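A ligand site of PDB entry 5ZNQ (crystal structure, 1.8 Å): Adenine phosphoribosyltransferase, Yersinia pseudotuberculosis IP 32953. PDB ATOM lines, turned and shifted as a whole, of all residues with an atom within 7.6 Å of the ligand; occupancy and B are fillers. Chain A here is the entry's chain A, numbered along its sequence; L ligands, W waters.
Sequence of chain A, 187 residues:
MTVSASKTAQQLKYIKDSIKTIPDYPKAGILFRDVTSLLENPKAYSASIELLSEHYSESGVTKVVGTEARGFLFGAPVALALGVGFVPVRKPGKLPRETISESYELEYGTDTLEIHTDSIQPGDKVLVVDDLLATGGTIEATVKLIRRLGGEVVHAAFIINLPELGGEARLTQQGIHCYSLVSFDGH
Ile 30 touches the ligand. CE1 of Phe 32 touches C4 of the ligand, at 3.4 Å. Leu 132 touches the ligand. Leu 162 touches the ligand (CD1 to C2, 3.4 Å). Leu 165 touches the ligand. Hydrophobic or aromatic side chains that line the ligand: Ile 30, Phe 32, Leu 132, Leu 162 and Leu 165. Of the 24 residues printed, 8 come within 4 Å of the ligand.
Water W3 lies within hydrogen-bond range of O of Asp 185 (2.8 Å), NE of Arg 33 (3.0 Å), N3 of the ligand (3.3 Å) and O of His 187 (3.4 Å).
NH1 of Arg 33 lies within hydrogen-bond range of O of Asp 185. O of Ile 30 lies within hydrogen-bond range of N of Tyr 25 (3.3 Å). N of Leu 162 sits at hydrogen-bond distance from O of Leu 133, 3.0 Å away. The backbone carbonyl oxygen (O) of Phe 32 is in hydrogen-bond range of the backbone NH (N) of Ile 22 (2.8 Å). O of Leu 31 sits at hydrogen-bond distance from NE of Arg 33, 3.3 Å away.
The backbone NH of Arg 33 lies within hydrogen-bond range of a nitrogen (N4) of the ligand (2.9 Å). The backbone carbonyl oxygen (O) of Leu 31 lies within hydrogen-bond range of a nitrogen (N3) of the ligand (2.9 Å). OXT of His 187 lies within hydrogen-bond range of N2 of the ligand (2.7 Å).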
ATOM      1  N   LYS A  20      -9.994  -2.161   5.858  1.00  0.00           N
ATOM      2  CA  LYS A  20     -11.226  -1.662   5.249  1.00  0.00           C
ATOM      3  C   LYS A  20     -11.933  -0.790   6.259  1.00  0.00           C
ATOM      4  O   LYS A  20     -11.753  -0.938   7.462  1.00  0.00           O
ATOM      5  CB  LYS A  20     -12.129  -2.803   4.752  1.00  0.00           C
ATOM      6  CG  LYS A  20     -11.544  -3.544   3.548  1.00  0.00           C
ATOM      7  CD  LYS A  20     -12.072  -4.989   3.500  1.00  0.00           C
ATOM      8  CE  LYS A  20     -12.404  -5.510   2.107  1.00  0.00           C
ATOM      9  NZ  LYS A  20     -13.739  -5.088   1.625  1.00  0.00           N
ATOM     10  N   ILE A  22     -15.612   0.793   7.541  1.00  0.00           N
ATOM     11  CA  ILE A  22     -17.033   0.528   7.572  1.00  0.00           C
ATOM     12  C   ILE A  22     -17.725   1.824   7.982  1.00  0.00           C
ATOM     13  O   ILE A  22     -17.671   2.199   9.173  1.00  0.00           O
ATOM     14  CB  ILE A  22     -17.414  -0.607   8.572  1.00  0.00           C
ATOM     15  CG1 ILE A  22     -16.549  -1.878   8.465  1.00  0.00           C
ATOM     16  CG2 ILE A  22     -18.910  -0.950   8.424  1.00  0.00           C
ATOM     17  CD1 ILE A  22     -16.874  -2.818   7.323  1.00  0.00           C
ATOM     18  N   TYR A  25     -20.543   2.777  11.519  1.00  0.00           N
ATOM     19  CA  TYR A  25     -20.501   1.623  12.401  1.00  0.00           C
ATOM     20  C   TYR A  25     -19.484   1.976  13.476  1.00  0.00           C
ATOM     21  O   TYR A  25     -18.403   2.480  13.136  1.00  0.00           O
ATOM     22  CB  TYR A  25     -20.113   0.344  11.627  1.00  0.00           C
ATOM     23  CG  TYR A  25     -19.961  -0.804  12.580  1.00  0.00           C
ATOM     24  CD1 TYR A  25     -18.786  -0.961  13.318  1.00  0.00           C
ATOM     25  CD2 TYR A  25     -20.997  -1.701  12.795  1.00  0.00           C
ATOM     26  CE1 TYR A  25     -18.625  -2.001  14.213  1.00  0.00           C
ATOM     27  CE2 TYR A  25     -20.843  -2.732  13.703  1.00  0.00           C
ATOM     28  CZ  TYR A  25     -19.670  -2.867  14.411  1.00  0.00           C
ATOM     29  OH  TYR A  25     -19.531  -3.859  15.302  1.00  0.00           O
ATOM     30  N   PRO A  26     -19.782   1.798  14.773  1.00  0.00           N
ATOM     31  CA  PRO A  26     -20.992   1.120  15.289  1.00  0.00           C
ATOM     32  C   PRO A  26     -22.203   2.024  15.444  1.00  0.00           C
ATOM     33  O   PRO A  26     -23.273   1.528  15.784  1.00  0.00           O
ATOM     34  CB  PRO A  26     -20.571   0.654  16.687  1.00  0.00           C
ATOM     35  CG  PRO A  26     -19.404   1.535  17.049  1.00  0.00           C
ATOM     36  CD  PRO A  26     -18.706   1.866  15.763  1.00  0.00           C
ATOM     37  N   GLY A  29     -21.952   8.253  11.773  1.00  0.00           N
ATOM     38  CA  GLY A  29     -20.837   9.186  11.840  1.00  0.00           C
ATOM     39  C   GLY A  29     -19.458   8.571  12.060  1.00  0.00           C
ATOM     40  O   GLY A  29     -18.452   9.140  11.672  1.00  0.00           O
ATOM     41  N   ILE A  30     -19.396   7.386  12.668  1.00  0.00           N
ATOM     42  CA  ILE A  30     -18.111   6.719  12.899  1.00  0.00           C
ATOM     43  C   ILE A  30     -17.647   5.963  11.639  1.00  0.00           C
ATOM     44  O   ILE A  30     -18.397   5.208  11.070  1.00  0.00           O
ATOM     45  CB  ILE A  30     -18.192   5.733  14.066  1.00  0.00           C
ATOM     46  CG1 ILE A  30     -18.670   6.451  15.337  1.00  0.00           C
ATOM     47  CG2 ILE A  30     -16.812   5.106  14.295  1.00  0.00           C
ATOM     48  CD1 ILE A  30     -17.703   7.513  15.811  1.00  0.00           C
ATOM     49  N   LEU A  31     -16.405   6.193  11.227  1.00  0.00           N
ATOM     50  CA  LEU A  31     -15.800   5.427  10.160  1.00  0.00           C
ATOM     51  C   LEU A  31     -14.976   4.338  10.812  1.00  0.00           C
ATOM     52  O   LEU A  31     -13.843   4.592  11.214  1.00  0.00           O
ATOM     53  CB  LEU A  31     -14.869   6.307   9.358  1.00  0.00           C
ATOM     54  CG  LEU A  31     -15.634   7.455   8.659  1.00  0.00           C
ATOM     55  CD1 LEU A  31     -14.678   8.464   8.067  1.00  0.00           C
ATOM     56  CD2 LEU A  31     -16.508   6.844   7.589  1.00  0.00           C
ATOM     57  N   PHE A  32     -15.511   3.119  10.882  1.00  0.00           N
ATOM     58  CA  PHE A  32     -14.811   2.061  11.595  1.00  0.00           C
ATOM     59  C   PHE A  32     -13.672   1.503  10.775  1.00  0.00           C
ATOM     60  O   PHE A  32     -13.822   1.232   9.597  1.00  0.00           O
ATOM     61  CB  PHE A  32     -15.811   0.944  11.947  1.00  0.00           C
ATOM     62  CG  PHE A  32     -15.288  -0.059  12.925  1.00  0.00           C
ATOM     63  CD1 PHE A  32     -15.399   0.150  14.285  1.00  0.00           C
ATOM     64  CD2 PHE A  32     -14.725  -1.268  12.508  1.00  0.00           C
ATOM     65  CE1 PHE A  32     -14.935  -0.776  15.207  1.00  0.00           C
ATOM     66  CE2 PHE A  32     -14.260  -2.207  13.424  1.00  0.00           C
ATOM     67  CZ  PHE A  32     -14.385  -1.970  14.775  1.00  0.00           C
ATOM     68  N   ARG A  33     -12.509   1.341  11.407  1.00  0.00           N
ATOM     69  CA  ARG A  33     -11.370   0.790  10.672  1.00  0.00           C
ATOM     70  C   ARG A  33     -11.288  -0.652  11.129  1.00  0.00           C
ATOM     71  O   ARG A  33     -11.102  -0.878  12.268  1.00  0.00           O
ATOM     72  CB  ARG A  33     -10.050   1.573  10.970  1.00  0.00           C
ATOM     73  CG  ARG A  33     -10.166   3.097  11.103  1.00  0.00           C
ATOM     74  CD  ARG A  33     -10.742   3.759   9.859  1.00  0.00           C
ATOM     75  NE  ARG A  33     -10.841   5.217   9.954  1.00  0.00           N
ATOM     76  CZ  ARG A  33     -10.951   5.996   8.873  1.00  0.00           C
ATOM     77  NH1 ARG A  33     -11.027   7.317   8.978  1.00  0.00           N
ATOM     78  NH2 ARG A  33     -10.979   5.446   7.674  1.00  0.00           N
ATOM     79  N   ASP A  34     -11.521  -1.574  10.227  1.00  0.00           N
ATOM     80  CA  ASP A  34     -11.693  -2.971  10.482  1.00  0.00           C
ATOM     81  C   ASP A  34     -10.408  -3.726  10.259  1.00  0.00           C
ATOM     82  O   ASP A  34     -10.114  -4.038   9.127  1.00  0.00           O
ATOM     83  CB  ASP A  34     -12.789  -3.481   9.575  1.00  0.00           C
ATOM     84  CG  ASP A  34     -13.013  -4.944   9.714  1.00  0.00           C
ATOM     85  OD1 ASP A  34     -12.480  -5.519  10.688  1.00  0.00           O
ATOM     86  OD2 ASP A  34     -13.728  -5.509   8.854  1.00  0.00           O
ATOM     87  N   VAL A  35      -9.667  -4.012  11.339  1.00  0.00           N
ATOM     88  CA  VAL A  35      -8.386  -4.777  11.216  1.00  0.00           C
ATOM     89  C   VAL A  35      -8.560  -6.243  10.767  1.00  0.00           C
ATOM     90  O   VAL A  35      -7.596  -6.913  10.395  1.00  0.00           O
ATOM     91  CB  VAL A  35      -7.550  -4.675  12.537  1.00  0.00           C
ATOM     92  CG1 VAL A  35      -8.032  -5.642  13.595  1.00  0.00           C
ATOM     93  CG2 VAL A  35      -6.077  -4.906  12.303  1.00  0.00           C
ATOM     94  N   ARG A  70      -7.502  -9.019  20.512  1.00  0.00           N
ATOM     95  CA  ARG A  70      -6.824  -8.597  19.261  1.00  0.00           C
ATOM     96  C   ARG A  70      -5.352  -8.303  19.541  1.00  0.00           C
ATOM     97  O   ARG A  70      -4.510  -8.435  18.666  1.00  0.00           O
ATOM     98  CB  ARG A  70      -7.616  -7.474  18.529  1.00  0.00           C
ATOM     99  CG  ARG A  70      -8.995  -7.903  18.040  1.00  0.00           C
ATOM    100  CD  ARG A  70      -9.458  -7.146  16.783  1.00  0.00           C
ATOM    101  NE  ARG A  70     -10.732  -7.597  16.211  1.00  0.00           N
ATOM    102  CZ  ARG A  70     -11.919  -7.034  16.442  1.00  0.00           C
ATOM    103  NH1 ARG A  70     -13.034  -7.523  15.845  1.00  0.00           N
ATOM    104  NH2 ARG A  70     -12.022  -5.982  17.263  1.00  0.00           N
ATOM    105  N   ASP A 131      -3.753  -3.862  18.682  1.00  0.00           N
ATOM    106  CA  ASP A 131      -4.181  -3.582  17.341  1.00  0.00           C
ATOM    107  C   ASP A 131      -4.366  -2.081  17.070  1.00  0.00           C
ATOM    108  O   ASP A 131      -3.913  -1.528  16.065  1.00  0.00           O
ATOM    109  CB  ASP A 131      -5.441  -4.337  16.913  1.00  0.00           C
ATOM    110  CG  ASP A 131      -6.656  -4.099  17.814  1.00  0.00           C
ATOM    111  OD1 ASP A 131      -6.578  -3.730  19.020  1.00  0.00           O
ATOM    112  OD2 ASP A 131      -7.771  -4.367  17.363  1.00  0.00           O
ATOM    113  N   LEU A 132      -5.061  -1.429  17.984  1.00  0.00           N
ATOM    114  CA  LEU A 132      -5.572  -0.111  17.726  1.00  0.00           C
ATOM    115  C   LEU A 132      -5.531   0.702  18.969  1.00  0.00           C
ATOM    116  O   LEU A 132      -6.089   0.286  19.999  1.00  0.00           O
ATOM    117  CB  LEU A 132      -6.986  -0.275  17.139  1.00  0.00           C
ATOM    118  CG  LEU A 132      -7.682   1.031  16.712  1.00  0.00           C
ATOM    119  CD1 LEU A 132      -8.606   0.734  15.520  1.00  0.00           C
ATOM    120  CD2 LEU A 132      -8.322   1.735  17.870  1.00  0.00           C
ATOM    121  N   LEU A 133      -4.974   1.922  18.835  1.00  0.00           N
ATOM    122  CA  LEU A 133      -4.959   2.899  19.945  1.00  0.00           C
ATOM    123  C   LEU A 133      -6.083   3.867  19.819  1.00  0.00           C
ATOM    124  O   LEU A 133      -6.095   4.652  18.909  1.00  0.00           O
ATOM    125  CB  LEU A 133      -3.625   3.713  19.986  1.00  0.00           C
ATOM    126  CG  LEU A 133      -3.330   4.607  21.202  1.00  0.00           C
ATOM    127  CD1 LEU A 133      -3.601   3.895  22.554  1.00  0.00           C
ATOM    128  CD2 LEU A 133      -1.914   5.129  21.145  1.00  0.00           C
ATOM    129  N   ALA A 134      -7.034   3.779  20.738  1.00  0.00           N
ATOM    130  CA  ALA A 134      -8.178   4.704  20.765  1.00  0.00           C
ATOM    131  C   ALA A 134      -8.063   5.529  22.028  1.00  0.00           C
ATOM    132  O   ALA A 134      -7.180   6.343  22.089  1.00  0.00           O
ATOM    133  CB  ALA A 134      -9.493   3.938  20.628  1.00  0.00           C
ATOM    134  N   THR A 135      -8.849   5.288  23.080  1.00  0.00           N
ATOM    135  CA  THR A 135      -8.669   6.099  24.302  1.00  0.00           C
ATOM    136  C   THR A 135      -7.420   5.677  25.196  1.00  0.00           C
ATOM    137  O   THR A 135      -6.985   6.478  26.072  1.00  0.00           O
ATOM    138  CB  THR A 135      -9.898   6.074  25.173  1.00  0.00           C
ATOM    139  OG1 THR A 135     -10.091   4.745  25.678  1.00  0.00           O
ATOM    140  CG2 THR A 135     -11.152   6.618  24.370  1.00  0.00           C
ATOM    141  N   ILE A 160      -2.867   0.498  14.261  1.00  0.00           N
ATOM    142  CA  ILE A 160      -3.627   1.733  13.953  1.00  0.00           C
ATOM    143  C   ILE A 160      -3.673   2.678  15.136  1.00  0.00           C
ATOM    144  O   ILE A 160      -3.955   2.228  16.283  1.00  0.00           O
ATOM    145  CB  ILE A 160      -5.103   1.355  13.637  1.00  0.00           C
ATOM    146  CG1 ILE A 160      -5.140   0.363  12.422  1.00  0.00           C
ATOM    147  CG2 ILE A 160      -6.000   2.579  13.493  1.00  0.00           C
ATOM    148  CD1 ILE A 160      -6.460  -0.348  12.203  1.00  0.00           C
ATOM    149  N   LEU A 162      -5.669   6.233  16.435  1.00  0.00           N
ATOM    150  CA  LEU A 162      -6.707   7.271  16.276  1.00  0.00           C
ATOM    151  C   LEU A 162      -6.430   8.430  17.202  1.00  0.00           C
ATOM    152  O   LEU A 162      -6.991   8.539  18.285  1.00  0.00           O
ATOM    153  CB  LEU A 162      -8.094   6.682  16.494  1.00  0.00           C
ATOM    154  CG  LEU A 162      -8.425   5.413  15.739  1.00  0.00           C
ATOM    155  CD1 LEU A 162      -9.839   4.952  16.047  1.00  0.00           C
ATOM    156  CD2 LEU A 162      -8.219   5.655  14.260  1.00  0.00           C
ATOM    157  N   LEU A 165      -8.728  10.447  19.532  1.00  0.00           N
ATOM    158  CA  LEU A 165      -9.307   9.873  20.773  1.00  0.00           C
ATOM    159  C   LEU A 165      -8.474  10.022  22.076  1.00  0.00           C
ATOM    160  O   LEU A 165      -8.929   9.619  23.176  1.00  0.00           O
ATOM    161  CB  LEU A 165      -9.643   8.415  20.507  1.00  0.00           C
ATOM    162  CG  LEU A 165     -10.842   8.300  19.577  1.00  0.00           C
ATOM    163  CD1 LEU A 165     -11.289   6.848  19.395  1.00  0.00           C
ATOM    164  CD2 LEU A 165     -11.991   9.166  20.068  1.00  0.00           C
ATOM    165  N   PHE A 184      -5.324   7.128  11.404  1.00  0.00           N
ATOM    166  CA  PHE A 184      -6.491   7.679  10.763  1.00  0.00           C
ATOM    167  C   PHE A 184      -7.054   8.840  11.574  1.00  0.00           C
ATOM    168  O   PHE A 184      -6.895   8.937  12.787  1.00  0.00           O
ATOM    169  CB  PHE A 184      -7.610   6.656  10.604  1.00  0.00           C
ATOM    170  CG  PHE A 184      -7.276   5.458   9.767  1.00  0.00           C
ATOM    171  CD1 PHE A 184      -7.530   5.463   8.391  1.00  0.00           C
ATOM    172  CD2 PHE A 184      -6.760   4.311  10.324  1.00  0.00           C
ATOM    173  CE1 PHE A 184      -7.301   4.352   7.632  1.00  0.00           C
ATOM    174  CE2 PHE A 184      -6.541   3.191   9.566  1.00  0.00           C
ATOM    175  CZ  PHE A 184      -6.780   3.211   8.209  1.00  0.00           C
ATOM    176  N   ASP A 185      -7.722   9.726  10.846  1.00  0.00           N
ATOM    177  CA  ASP A 185      -8.536  10.747  11.397  1.00  0.00           C
ATOM    178  C   ASP A 185      -9.882  10.171  11.842  1.00  0.00           C
ATOM    179  O   ASP A 185     -10.325   9.070  11.421  1.00  0.00           O
ATOM    180  CB  ASP A 185      -8.814  11.802  10.288  1.00  0.00           C
ATOM    181  CG  ASP A 185      -7.559  12.566   9.865  1.00  0.00           C
ATOM    182  OD1 ASP A 185      -6.674  12.764  10.731  1.00  0.00           O
ATOM    183  OD2 ASP A 185      -7.514  13.009   8.675  1.00  0.00           O
ATOM    184  N   GLY A 186     -10.530  10.950  12.696  1.00  0.00           N
ATOM    185  CA  GLY A 186     -11.875  10.639  13.177  1.00  0.00           C
ATOM    186  C   GLY A 186     -11.864   9.953  14.520  1.00  0.00           C
ATOM    187  O   GLY A 186     -10.809   9.695  15.088  1.00  0.00           O
ATOM    188  N   HIS A 187     -13.071   9.654  15.001  1.00  0.00           N
ATOM    189  CA  HIS A 187     -13.303   9.023  16.303  1.00  0.00           C
ATOM    190  C   HIS A 187     -13.613   7.528  16.118  1.00  0.00           C
ATOM    191  O   HIS A 187     -13.651   7.040  14.985  1.00  0.00           O
ATOM    192  CB  HIS A 187     -14.458   9.706  17.057  1.00  0.00           C
ATOM    193  CG  HIS A 187     -14.101  11.071  17.585  1.00  0.00           C
ATOM    194  ND1 HIS A 187     -14.571  11.542  18.796  1.00  0.00           N
ATOM    195  CD2 HIS A 187     -13.323  12.055  17.080  1.00  0.00           C
ATOM    196  CE1 HIS A 187     -14.093  12.762  19.010  1.00  0.00           C
ATOM    197  NE2 HIS A 187     -13.331  13.089  17.987  1.00  0.00           N
ATOM    198  OXT HIS A 187     -13.835   6.841  17.113  1.00  0.00           O
HETATM  199  N1  LIG L   1     -12.585   2.359  18.216  1.00  0.00           N
HETATM  200  C1  LIG L   1     -12.970   3.634  18.380  1.00  0.00           C
HETATM  201  N2  LIG L   1     -13.150   4.281  17.203  1.00  0.00           N
HETATM  202  C2  LIG L   1     -12.847   3.386  16.236  1.00  0.00           C
HETATM  203  C3  LIG L   1     -12.799   3.365  14.770  1.00  0.00           C
HETATM  204  N3  LIG L   1     -13.107   4.451  14.049  1.00  0.00           N
HETATM  205  N4  LIG L   1     -12.425   2.192  14.180  1.00  0.00           N
HETATM  206  C4  LIG L   1     -12.103   1.087  14.846  1.00  0.00           C
HETATM  207  N5  LIG L   1     -12.105   1.032  16.169  1.00  0.00           N
HETATM  208  C5  LIG L   1     -12.450   2.135  16.907  1.00  0.00           C
HETATM  209  O   HOH W   1     -12.053   0.953  20.473  1.00  0.00           O
HETATM  210  O   HOH W   2     -11.522  -1.224  17.732  1.00  0.00           O
HETATM  211  O   HOH W   3     -11.341   6.739  12.525  1.00  0.00           O
